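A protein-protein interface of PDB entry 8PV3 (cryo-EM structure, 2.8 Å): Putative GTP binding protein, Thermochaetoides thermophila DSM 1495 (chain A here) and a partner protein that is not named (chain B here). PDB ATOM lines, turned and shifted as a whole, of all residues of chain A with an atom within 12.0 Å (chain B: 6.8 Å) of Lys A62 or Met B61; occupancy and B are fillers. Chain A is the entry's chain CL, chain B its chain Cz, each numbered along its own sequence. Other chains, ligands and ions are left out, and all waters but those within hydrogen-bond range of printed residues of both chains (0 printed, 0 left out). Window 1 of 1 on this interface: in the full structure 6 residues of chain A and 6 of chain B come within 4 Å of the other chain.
OD1 of Asn A57 sits at hydrogen-bond distance from NZ of Lys B62 (3.3 Å).
NZ of Lys A62 is in salt-bridge range of OE2 of Glu B65 (3.2 Å).
The backbone NH (N) of Gln A67 lies close to the side-chain amino group (NZ) of Lys B64 (3.3 Å).
The backbone carbonyl oxygen (O) of Ile A55 lies within hydrogen-bond range of the side-chain amino group (NZ) of Lys A62.
The side-chain amino group (NZ) of Lys A62 is in hydrogen-bond range of the side-chain amide oxygen (OD1) of Asn A57 (2.7 Å).
NZ of Lys B62 lies within salt-bridge range of OE1 of Glu B65, 2.7 Å away.
OE2 of Glu B65 is in salt-bridge range of NZ of Lys B69, 3.3 Å away.
Among the printed residues, merely in contact across the chains: Asn A57 with Gln B58, Asn A57 with Met B61, Asn A57 with Glu B65, Lys A62 with Met B61, Glu A63 with Met B61, Glu A63 with Lys B64 and Leu A66 with Lys B64.
Lys A62 touches just these residues of chain B: Met B61 and Glu B65.
Gln B58 touches one residue of chain A.
No residue of chain A comes within 4 Å of Ala B59.
No residue of chain A comes within 4 Å of Ala B60.
Lys B62 touches one residue of chain A.
Ala B63 touches none of the printed residues of chain A.
Glu B65 touches just these residues of chain A: Asn A57 and Lys A62.
Printed residues of chain B within 4 Å of Gln A67: Lys B64 (3.3 Å).
Printed residues of chain B within 4 Å of Glu A63: Met B61 and Lys B64.
Of the printed residues of chain B, Leu A66 touches Lys B64.
Arg B66 touches none of the printed residues of chain A.
Glu A71 touches none of the printed residues of chain B.
Along chain B the printed residues that touch a printed residue of chain A span positions 58 to 65.
Of the 21 printed residues of chain A, 5 touch a printed residue of chain B.
Hydrophobic or aromatic side chains of chain A that line the printed part of chain B: Leu A66.
Among the printed residues, Asp or Glu carboxylates within 4 Å of a Lys or Arg side-chain nitrogen of the other chain: Lys A62 with Glu B65 (3.2 Å).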
ATOM      1  N   ASP A  52      -9.567 -13.812 -28.635  1.00  0.00           N
ATOM      2  CA  ASP A  52      -8.843 -14.993 -28.193  1.00  0.00           C
ATOM      3  C   ASP A  52      -9.279 -16.200 -29.023  1.00  0.00           C
ATOM      4  O   ASP A  52     -10.477 -16.396 -29.248  1.00  0.00           O
ATOM      5  CB  ASP A  52      -9.092 -15.237 -26.701  1.00  0.00           C
ATOM      6  CG  ASP A  52      -8.281 -16.399 -26.134  1.00  0.00           C
ATOM      7  OD1 ASP A  52      -7.470 -16.141 -25.221  1.00  0.00           O
ATOM      8  OD2 ASP A  52      -8.474 -17.564 -26.537  1.00  0.00           O
ATOM      9  N   PRO A  53      -8.330 -17.011 -29.499  1.00  0.00           N
ATOM     10  CA  PRO A  53      -8.698 -18.158 -30.346  1.00  0.00           C
ATOM     11  C   PRO A  53      -9.457 -19.255 -29.613  1.00  0.00           C
ATOM     12  O   PRO A  53     -10.229 -19.980 -30.252  1.00  0.00           O
ATOM     13  CB  PRO A  53      -7.343 -18.663 -30.859  1.00  0.00           C
ATOM     14  CG  PRO A  53      -6.383 -17.537 -30.628  1.00  0.00           C
ATOM     15  CD  PRO A  53      -6.872 -16.843 -29.401  1.00  0.00           C
ATOM     16  N   GLY A  54      -9.270 -19.405 -28.306  1.00  0.00           N
ATOM     17  CA  GLY A  54     -10.016 -20.390 -27.546  1.00  0.00           C
ATOM     18  C   GLY A  54      -9.242 -21.672 -27.302  1.00  0.00           C
ATOM     19  O   GLY A  54      -8.009 -21.712 -27.308  1.00  0.00           O
ATOM     20  N   ILE A  55      -9.995 -22.738 -27.077  1.00  0.00           N
ATOM     21  CA  ILE A  55      -9.445 -24.071 -26.837  1.00  0.00           C
ATOM     22  C   ILE A  55      -9.608 -24.890 -28.113  1.00  0.00           C
ATOM     23  O   ILE A  55     -10.694 -24.869 -28.708  1.00  0.00           O
ATOM     24  CB  ILE A  55     -10.141 -24.766 -25.654  1.00  0.00           C
ATOM     25  CG1 ILE A  55     -10.337 -23.786 -24.498  1.00  0.00           C
ATOM     26  CG2 ILE A  55      -9.341 -25.968 -25.190  1.00  0.00           C
ATOM     27  CD1 ILE A  55     -11.326 -24.264 -23.463  1.00  0.00           C
ATOM     28  N   PRO A  56      -8.571 -25.591 -28.573  1.00  0.00           N
ATOM     29  CA  PRO A  56      -8.717 -26.435 -29.767  1.00  0.00           C
ATOM     30  C   PRO A  56      -9.662 -27.600 -29.513  1.00  0.00           C
ATOM     31  O   PRO A  56      -9.752 -28.118 -28.400  1.00  0.00           O
ATOM     32  CB  PRO A  56      -7.287 -26.919 -30.035  1.00  0.00           C
ATOM     33  CG  PRO A  56      -6.410 -25.959 -29.321  1.00  0.00           C
ATOM     34  CD  PRO A  56      -7.176 -25.537 -28.111  1.00  0.00           C
ATOM     35  N   ASN A  57     -10.362 -28.018 -30.571  1.00  0.00           N
ATOM     36  CA  ASN A  57     -11.337 -29.096 -30.440  1.00  0.00           C
ATOM     37  C   ASN A  57     -10.659 -30.438 -30.203  1.00  0.00           C
ATOM     38  O   ASN A  57     -11.230 -31.324 -29.557  1.00  0.00           O
ATOM     39  CB  ASN A  57     -12.217 -29.158 -31.686  1.00  0.00           C
ATOM     40  CG  ASN A  57     -13.071 -27.922 -31.855  1.00  0.00           C
ATOM     41  OD1 ASN A  57     -13.430 -27.263 -30.882  1.00  0.00           O
ATOM     42  ND2 ASN A  57     -13.403 -27.601 -33.099  1.00  0.00           N
ATOM     43  N   LEU A  58      -9.438 -30.610 -30.712  1.00  0.00           N
ATOM     44  CA  LEU A  58      -8.768 -31.901 -30.609  1.00  0.00           C
ATOM     45  C   LEU A  58      -8.141 -32.132 -29.242  1.00  0.00           C
ATOM     46  O   LEU A  58      -7.604 -33.218 -29.001  1.00  0.00           O
ATOM     47  CB  LEU A  58      -7.701 -32.041 -31.696  1.00  0.00           C
ATOM     48  CG  LEU A  58      -8.106 -32.797 -32.966  1.00  0.00           C
ATOM     49  CD1 LEU A  58      -9.239 -32.102 -33.706  1.00  0.00           C
ATOM     50  CD2 LEU A  58      -6.909 -33.000 -33.877  1.00  0.00           C
ATOM     51  N   PHE A  59      -8.177 -31.143 -28.356  1.00  0.00           N
ATOM     52  CA  PHE A  59      -7.725 -31.332 -26.989  1.00  0.00           C
ATOM     53  C   PHE A  59      -8.661 -32.310 -26.279  1.00  0.00           C
ATOM     54  O   PHE A  59      -9.877 -32.071 -26.239  1.00  0.00           O
ATOM     55  CB  PHE A  59      -7.686 -29.993 -26.257  1.00  0.00           C
ATOM     56  CG  PHE A  59      -7.073 -30.067 -24.892  1.00  0.00           C
ATOM     57  CD1 PHE A  59      -5.765 -30.492 -24.730  1.00  0.00           C
ATOM     58  CD2 PHE A  59      -7.801 -29.708 -23.771  1.00  0.00           C
ATOM     59  CE1 PHE A  59      -5.196 -30.564 -23.475  1.00  0.00           C
ATOM     60  CE2 PHE A  59      -7.237 -29.777 -22.513  1.00  0.00           C
ATOM     61  CZ  PHE A  59      -5.934 -30.206 -22.365  1.00  0.00           C
ATOM     62  N   PRO A  60      -8.147 -33.415 -25.732  1.00  0.00           N
ATOM     63  CA  PRO A  60      -9.040 -34.489 -25.262  1.00  0.00           C
ATOM     64  C   PRO A  60      -9.837 -34.149 -24.016  1.00  0.00           C
ATOM     65  O   PRO A  60     -10.800 -34.861 -23.708  1.00  0.00           O
ATOM     66  CB  PRO A  60      -8.075 -35.656 -24.998  1.00  0.00           C
ATOM     67  CG  PRO A  60      -6.824 -35.307 -25.730  1.00  0.00           C
ATOM     68  CD  PRO A  60      -6.734 -33.820 -25.679  1.00  0.00           C
ATOM     69  N   TYR A  61      -9.475 -33.097 -23.286  1.00  0.00           N
ATOM     70  CA  TYR A  61     -10.158 -32.732 -22.052  1.00  0.00           C
ATOM     71  C   TYR A  61     -10.770 -31.337 -22.131  1.00  0.00           C
ATOM     72  O   TYR A  61     -10.862 -30.631 -21.122  1.00  0.00           O
ATOM     73  CB  TYR A  61      -9.196 -32.840 -20.873  1.00  0.00           C
ATOM     74  CG  TYR A  61      -8.485 -34.172 -20.816  1.00  0.00           C
ATOM     75  CD1 TYR A  61      -9.197 -35.363 -20.865  1.00  0.00           C
ATOM     76  CD2 TYR A  61      -7.102 -34.240 -20.733  1.00  0.00           C
ATOM     77  CE1 TYR A  61      -8.553 -36.582 -20.821  1.00  0.00           C
ATOM     78  CE2 TYR A  61      -6.450 -35.456 -20.691  1.00  0.00           C
ATOM     79  CZ  TYR A  61      -7.180 -36.623 -20.735  1.00  0.00           C
ATOM     80  OH  TYR A  61      -6.534 -37.835 -20.690  1.00  0.00           O
ATOM     81  N   LYS A  62     -11.198 -30.935 -23.332  1.00  0.00           N
ATOM     82  CA  LYS A  62     -11.786 -29.612 -23.515  1.00  0.00           C
ATOM     83  C   LYS A  62     -13.122 -29.489 -22.795  1.00  0.00           C
ATOM     84  O   LYS A  62     -13.417 -28.447 -22.200  1.00  0.00           O
ATOM     85  CB  LYS A  62     -11.944 -29.312 -25.006  1.00  0.00           C
ATOM     86  CG  LYS A  62     -12.607 -27.978 -25.303  1.00  0.00           C
ATOM     87  CD  LYS A  62     -12.525 -27.621 -26.771  1.00  0.00           C
ATOM     88  CE  LYS A  62     -13.276 -26.339 -27.061  1.00  0.00           C
ATOM     89  NZ  LYS A  62     -13.195 -25.957 -28.493  1.00  0.00           N
ATOM     90  N   GLU A  63     -13.941 -30.544 -22.831  1.00  0.00           N
ATOM     91  CA  GLU A  63     -15.227 -30.516 -22.138  1.00  0.00           C
ATOM     92  C   GLU A  63     -15.037 -30.410 -20.630  1.00  0.00           C
ATOM     93  O   GLU A  63     -15.744 -29.650 -19.955  1.00  0.00           O
ATOM     94  CB  GLU A  63     -16.041 -31.759 -22.491  1.00  0.00           C
ATOM     95  CG  GLU A  63     -17.439 -31.770 -21.898  1.00  0.00           C
ATOM     96  CD  GLU A  63     -18.123 -33.113 -22.047  1.00  0.00           C
ATOM     97  OE1 GLU A  63     -17.473 -34.061 -22.533  1.00  0.00           O
ATOM     98  OE2 GLU A  63     -19.311 -33.219 -21.677  1.00  0.00           O
ATOM     99  N   ARG A  64     -14.069 -31.150 -20.087  1.00  0.00           N
ATOM    100  CA  ARG A  64     -13.762 -31.035 -18.665  1.00  0.00           C
ATOM    101  C   ARG A  64     -13.257 -29.641 -18.321  1.00  0.00           C
ATOM    102  O   ARG A  64     -13.656 -29.070 -17.300  1.00  0.00           O
ATOM    103  CB  ARG A  64     -12.737 -32.090 -18.254  1.00  0.00           C
ATOM    104  CG  ARG A  64     -13.142 -33.514 -18.568  1.00  0.00           C
ATOM    105  CD  ARG A  64     -12.545 -34.474 -17.555  1.00  0.00           C
ATOM    106  NE  ARG A  64     -11.162 -34.144 -17.236  1.00  0.00           N
ATOM    107  CZ  ARG A  64     -10.140 -34.972 -17.396  1.00  0.00           C
ATOM    108  NH1 ARG A  64     -10.311 -36.200 -17.856  1.00  0.00           N
ATOM    109  NH2 ARG A  64      -8.915 -34.557 -17.083  1.00  0.00           N
ATOM    110  N   LEU A  65     -12.400 -29.071 -19.175  1.00  0.00           N
ATOM    111  CA  LEU A  65     -11.881 -27.728 -18.933  1.00  0.00           C
ATOM    112  C   LEU A  65     -13.001 -26.695 -18.943  1.00  0.00           C
ATOM    113  O   LEU A  65     -13.007 -25.762 -18.127  1.00  0.00           O
ATOM    114  CB  LEU A  65     -10.815 -27.392 -19.975  1.00  0.00           C
ATOM    115  CG  LEU A  65      -9.992 -26.120 -19.777  1.00  0.00           C
ATOM    116  CD1 LEU A  65      -9.470 -26.045 -18.358  1.00  0.00           C
ATOM    117  CD2 LEU A  65      -8.845 -26.081 -20.767  1.00  0.00           C
ATOM    118  N   LEU A  66     -13.981 -26.871 -19.832  1.00  0.00           N
ATOM    119  CA  LEU A  66     -15.172 -26.027 -19.800  1.00  0.00           C
ATOM    120  C   LEU A  66     -15.979 -26.253 -18.526  1.00  0.00           C
ATOM    121  O   LEU A  66     -16.635 -25.329 -18.032  1.00  0.00           O
ATOM    122  CB  LEU A  66     -16.035 -26.279 -21.034  1.00  0.00           C
ATOM    123  CG  LEU A  66     -15.414 -25.897 -22.379  1.00  0.00           C
ATOM    124  CD1 LEU A  66     -16.373 -26.191 -23.522  1.00  0.00           C
ATOM    125  CD2 LEU A  66     -14.996 -24.439 -22.376  1.00  0.00           C
ATOM    126  N   GLN A  67     -15.944 -27.473 -17.979  1.00  0.00           N
ATOM    127  CA  GLN A  67     -16.609 -27.715 -16.697  1.00  0.00           C
ATOM    128  C   GLN A  67     -15.949 -26.931 -15.563  1.00  0.00           C
ATOM    129  O   GLN A  67     -16.650 -26.345 -14.728  1.00  0.00           O
ATOM    130  CB  GLN A  67     -16.653 -29.209 -16.365  1.00  0.00           C
ATOM    131  CG  GLN A  67     -17.526 -30.038 -17.287  1.00  0.00           C
ATOM    132  CD  GLN A  67     -17.523 -31.510 -16.931  1.00  0.00           C
ATOM    133  OE1 GLN A  67     -16.811 -31.938 -16.023  1.00  0.00           O
ATOM    134  NE2 GLN A  67     -18.319 -32.292 -17.647  1.00  0.00           N
ATOM    135  N   GLN A  68     -14.607 -26.897 -15.502  1.00  0.00           N
ATOM    136  CA  GLN A  68     -14.002 -26.055 -14.460  1.00  0.00           C
ATOM    137  C   GLN A  68     -14.229 -24.572 -14.735  1.00  0.00           C
ATOM    138  O   GLN A  68     -14.321 -23.777 -13.795  1.00  0.00           O
ATOM    139  CB  GLN A  68     -12.498 -26.273 -14.182  1.00  0.00           C
ATOM    140  CG  GLN A  68     -12.014 -27.593 -13.560  1.00  0.00           C
ATOM    141  CD  GLN A  68     -11.791 -28.709 -14.525  1.00  0.00           C
ATOM    142  OE1 GLN A  68     -11.660 -28.479 -15.712  1.00  0.00           O
ATOM    143  NE2 GLN A  68     -11.749 -29.936 -14.020  1.00  0.00           N
ATOM    144  N   ILE A  69     -14.317 -24.174 -16.009  1.00  0.00           N
ATOM    145  CA  ILE A  69     -14.617 -22.772 -16.321  1.00  0.00           C
ATOM    146  C   ILE A  69     -15.995 -22.387 -15.790  1.00  0.00           C
ATOM    147  O   ILE A  69     -16.160 -21.363 -15.107  1.00  0.00           O
ATOM    148  CB  ILE A  69     -14.509 -22.523 -17.837  1.00  0.00           C
ATOM    149  CG1 ILE A  69     -13.047 -22.528 -18.283  1.00  0.00           C
ATOM    150  CG2 ILE A  69     -15.179 -21.214 -18.223  1.00  0.00           C
ATOM    151  CD1 ILE A  69     -12.875 -22.457 -19.782  1.00  0.00           C
ATOM    152  N   GLU A  70     -16.996 -23.228 -16.067  1.00  0.00           N
ATOM    153  CA  GLU A  70     -18.353 -22.986 -15.584  1.00  0.00           C
ATOM    154  C   GLU A  70     -18.410 -22.996 -14.061  1.00  0.00           C
ATOM    155  O   GLU A  70     -19.029 -22.118 -13.447  1.00  0.00           O
ATOM    156  CB  GLU A  70     -19.300 -24.041 -16.162  1.00  0.00           C
ATOM    157  CG  GLU A  70     -20.764 -23.878 -15.765  1.00  0.00           C
ATOM    158  CD  GLU A  70     -21.405 -22.613 -16.305  1.00  0.00           C
ATOM    159  OE1 GLU A  70     -20.948 -22.102 -17.348  1.00  0.00           O
ATOM    160  OE2 GLU A  70     -22.372 -22.128 -15.681  1.00  0.00           O
ATOM    161  N   GLU A  71     -17.747 -23.974 -13.436  1.00  0.00           N
ATOM    162  CA  GLU A  71     -17.765 -24.091 -11.982  1.00  0.00           C
ATOM    163  C   GLU A  71     -17.092 -22.894 -11.323  1.00  0.00           C
ATOM    164  O   GLU A  71     -17.578 -22.372 -10.313  1.00  0.00           O
ATOM    165  CB  GLU A  71     -17.089 -25.398 -11.563  1.00  0.00           C
ATOM    166  CG  GLU A  71     -16.789 -25.511 -10.081  1.00  0.00           C
ATOM    167  CD  GLU A  71     -15.897 -26.690  -9.761  1.00  0.00           C
ATOM    168  OE1 GLU A  71     -15.415 -27.346 -10.709  1.00  0.00           O
ATOM    169  OE2 GLU A  71     -15.675 -26.962  -8.563  1.00  0.00           O
ATOM    170  N   ARG A  73     -16.798 -19.850 -12.614  1.00  0.00           N
ATOM    171  CA  ARG A  73     -17.621 -18.651 -12.765  1.00  0.00           C
ATOM    172  C   ARG A  73     -18.817 -18.668 -11.815  1.00  0.00           C
ATOM    173  O   ARG A  73     -19.188 -17.624 -11.263  1.00  0.00           O
ATOM    174  CB  ARG A  73     -18.082 -18.467 -14.211  1.00  0.00           C
ATOM    175  CG  ARG A  73     -16.955 -18.127 -15.172  1.00  0.00           C
ATOM    176  CD  ARG A  73     -17.473 -17.867 -16.578  1.00  0.00           C
ATOM    177  NE  ARG A  73     -17.994 -19.059 -17.232  1.00  0.00           N
ATOM    178  CZ  ARG A  73     -19.271 -19.237 -17.538  1.00  0.00           C
ATOM    179  NH1 ARG A  73     -20.186 -18.329 -17.242  1.00  0.00           N
ATOM    180  NH2 ARG A  73     -19.639 -20.352 -18.159  1.00  0.00           N
ATOM    181  N   GLN B  56     -19.725 -38.932 -30.681  1.00  0.00           N
ATOM    182  CA  GLN B  56     -20.768 -38.541 -29.729  1.00  0.00           C
ATOM    183  C   GLN B  56     -20.264 -37.506 -28.717  1.00  0.00           C
ATOM    184  O   GLN B  56     -20.921 -36.476 -28.496  1.00  0.00           O
ATOM    185  CB  GLN B  56     -21.338 -39.771 -29.025  1.00  0.00           C
ATOM    186  CG  GLN B  56     -22.057 -40.723 -29.968  1.00  0.00           C
ATOM    187  CD  GLN B  56     -22.440 -42.030 -29.305  1.00  0.00           C
ATOM    188  OE1 GLN B  56     -22.157 -42.249 -28.128  1.00  0.00           O
ATOM    189  NE2 GLN B  56     -23.086 -42.910 -30.061  1.00  0.00           N
ATOM    190  N   GLU B  57     -19.089 -37.740 -28.105  1.00  0.00           N
ATOM    191  CA  GLU B  57     -18.591 -36.700 -27.190  1.00  0.00           C
ATOM    192  C   GLU B  57     -18.189 -35.429 -27.931  1.00  0.00           C
ATOM    193  O   GLU B  57     -18.285 -34.334 -27.368  1.00  0.00           O
ATOM    194  CB  GLU B  57     -17.428 -37.106 -26.261  1.00  0.00           C
ATOM    195  CG  GLU B  57     -17.666 -38.130 -25.137  1.00  0.00           C
ATOM    196  CD  GLU B  57     -17.571 -39.564 -25.537  1.00  0.00           C
ATOM    197  OE1 GLU B  57     -17.240 -39.821 -26.688  1.00  0.00           O
ATOM    198  OE2 GLU B  57     -17.836 -40.438 -24.691  1.00  0.00           O
ATOM    199  N   GLN B  58     -17.742 -35.543 -29.184  1.00  0.00           N
ATOM    200  CA  GLN B  58     -17.412 -34.347 -29.950  1.00  0.00           C
ATOM    201  C   GLN B  58     -18.646 -33.489 -30.199  1.00  0.00           C
ATOM    202  O   GLN B  58     -18.602 -32.264 -30.023  1.00  0.00           O
ATOM    203  CB  GLN B  58     -16.764 -34.750 -31.272  1.00  0.00           C
ATOM    204  CG  GLN B  58     -16.304 -33.588 -32.125  1.00  0.00           C
ATOM    205  CD  GLN B  58     -15.164 -32.820 -31.491  1.00  0.00           C
ATOM    206  OE1 GLN B  58     -14.247 -33.409 -30.921  1.00  0.00           O
ATOM    207  NE2 GLN B  58     -15.213 -31.498 -31.588  1.00  0.00           N
ATOM    208  N   ALA B  59     -19.762 -34.119 -30.577  1.00  0.00           N
ATOM    209  CA  ALA B  59     -21.003 -33.382 -30.798  1.00  0.00           C
ATOM    210  C   ALA B  59     -21.514 -32.753 -29.508  1.00  0.00           C
ATOM    211  O   ALA B  59     -21.955 -31.593 -29.507  1.00  0.00           O
ATOM    212  CB  ALA B  59     -22.058 -34.307 -31.402  1.00  0.00           C
ATOM    213  N   ALA B  60     -21.449 -33.498 -28.397  1.00  0.00           N
ATOM    214  CA  ALA B  60     -21.889 -32.958 -27.111  1.00  0.00           C
ATOM    215  C   ALA B  60     -21.037 -31.765 -26.683  1.00  0.00           C
ATOM    216  O   ALA B  60     -21.562 -30.745 -26.211  1.00  0.00           O
ATOM    217  CB  ALA B  60     -21.851 -34.054 -26.047  1.00  0.00           C
ATOM    218  N   MET B  61     -19.716 -31.873 -26.857  1.00  0.00           N
ATOM    219  CA  MET B  61     -18.816 -30.791 -26.473  1.00  0.00           C
ATOM    220  C   MET B  61     -19.032 -29.556 -27.337  1.00  0.00           C
ATOM    221  O   MET B  61     -19.001 -28.427 -26.830  1.00  0.00           O
ATOM    222  CB  MET B  61     -17.367 -31.289 -26.545  1.00  0.00           C
ATOM    223  CG  MET B  61     -16.279 -30.307 -26.112  1.00  0.00           C
ATOM    224  SD  MET B  61     -15.740 -29.094 -27.337  1.00  0.00           S
ATOM    225  CE  MET B  61     -14.811 -30.138 -28.454  1.00  0.00           C
ATOM    226  N   LYS B  62     -19.252 -29.744 -28.643  1.00  0.00           N
ATOM    227  CA  LYS B  62     -19.498 -28.597 -29.513  1.00  0.00           C
ATOM    228  C   LYS B  62     -20.818 -27.915 -29.175  1.00  0.00           C
ATOM    229  O   LYS B  62     -20.911 -26.680 -29.210  1.00  0.00           O
ATOM    230  CB  LYS B  62     -19.480 -29.022 -30.982  1.00  0.00           C
ATOM    231  CG  LYS B  62     -18.111 -29.429 -31.510  1.00  0.00           C
ATOM    232  CD  LYS B  62     -17.070 -28.354 -31.246  1.00  0.00           C
ATOM    233  CE  LYS B  62     -17.314 -27.111 -32.086  1.00  0.00           C
ATOM    234  NZ  LYS B  62     -16.301 -26.054 -31.813  1.00  0.00           N
ATOM    235  N   ALA B  63     -21.846 -28.701 -28.835  1.00  0.00           N
ATOM    236  CA  ALA B  63     -23.120 -28.119 -28.422  1.00  0.00           C
ATOM    237  C   ALA B  63     -22.965 -27.294 -27.149  1.00  0.00           C
ATOM    238  O   ALA B  63     -23.484 -26.172 -27.054  1.00  0.00           O
ATOM    239  CB  ALA B  63     -24.160 -29.222 -28.228  1.00  0.00           C
ATOM    240  N   LYS B  64     -22.229 -27.827 -26.166  1.00  0.00           N
ATOM    241  CA  LYS B  64     -22.012 -27.087 -24.923  1.00  0.00           C
ATOM    242  C   LYS B  64     -21.211 -25.809 -25.163  1.00  0.00           C
ATOM    243  O   LYS B  64     -21.522 -24.753 -24.590  1.00  0.00           O
ATOM    244  CB  LYS B  64     -21.301 -27.971 -23.899  1.00  0.00           C
ATOM    245  CG  LYS B  64     -20.973 -27.244 -22.608  1.00  0.00           C
ATOM    246  CD  LYS B  64     -20.058 -28.042 -21.707  1.00  0.00           C
ATOM    247  CE  LYS B  64     -19.759 -27.261 -20.440  1.00  0.00           C
ATOM    248  NZ  LYS B  64     -18.837 -27.995 -19.543  1.00  0.00           N
ATOM    249  N   GLU B  65     -20.184 -25.885 -26.017  1.00  0.00           N
ATOM    250  CA  GLU B  65     -19.373 -24.711 -26.327  1.00  0.00           C
ATOM    251  C   GLU B  65     -20.199 -23.631 -27.016  1.00  0.00           C
ATOM    252  O   GLU B  65     -20.067 -22.441 -26.699  1.00  0.00           O
ATOM    253  CB  GLU B  65     -18.186 -25.115 -27.201  1.00  0.00           C
ATOM    254  CG  GLU B  65     -17.235 -23.976 -27.523  1.00  0.00           C
ATOM    255  CD  GLU B  65     -16.205 -24.355 -28.569  1.00  0.00           C
ATOM    256  OE1 GLU B  65     -16.339 -25.439 -29.173  1.00  0.00           O
ATOM    257  OE2 GLU B  65     -15.262 -23.566 -28.787  1.00  0.00           O
ATOM    258  N   ARG B  66     -21.070 -24.031 -27.948  1.00  0.00           N
ATOM    259  CA  ARG B  66     -21.911 -23.053 -28.629  1.00  0.00           C
ATOM    260  C   ARG B  66     -22.920 -22.427 -27.674  1.00  0.00           C
ATOM    261  O   ARG B  66     -23.208 -21.229 -27.774  1.00  0.00           O
ATOM    262  CB  ARG B  66     -22.619 -23.700 -29.820  1.00  0.00           C
ATOM    263  CG  ARG B  66     -23.416 -22.717 -30.662  1.00  0.00           C
ATOM    264  CD  ARG B  66     -24.046 -23.378 -31.876  1.00  0.00           C
ATOM    265  NE  ARG B  66     -25.043 -24.378 -31.517  1.00  0.00           N
ATOM    266  CZ  ARG B  66     -24.911 -25.677 -31.743  1.00  0.00           C
ATOM    267  NH1 ARG B  66     -23.832 -26.171 -32.328  1.00  0.00           N
ATOM    268  NH2 ARG B  66     -25.888 -26.503 -31.377  1.00  0.00           N
ATOM    269  N   LYS B  69     -20.978 -19.835 -25.630  1.00  0.00           N
ATOM    270  CA  LYS B  69     -20.711 -18.666 -26.462  1.00  0.00           C
ATOM    271  C   LYS B  69     -21.970 -17.833 -26.674  1.00  0.00           C
ATOM    272  O   LYS B  69     -21.906 -16.599 -26.683  1.00  0.00           O
ATOM    273  CB  LYS B  69     -20.125 -19.099 -27.805  1.00  0.00           C
ATOM    274  CG  LYS B  69     -18.683 -19.570 -27.729  1.00  0.00           C
ATOM    275  CD  LYS B  69     -18.182 -20.028 -29.089  1.00  0.00           C
ATOM    276  CE  LYS B  69     -16.689 -20.311 -29.059  1.00  0.00           C
ATOM    277  NZ  LYS B  69     -16.180 -20.812 -30.368  1.00  0.00           N
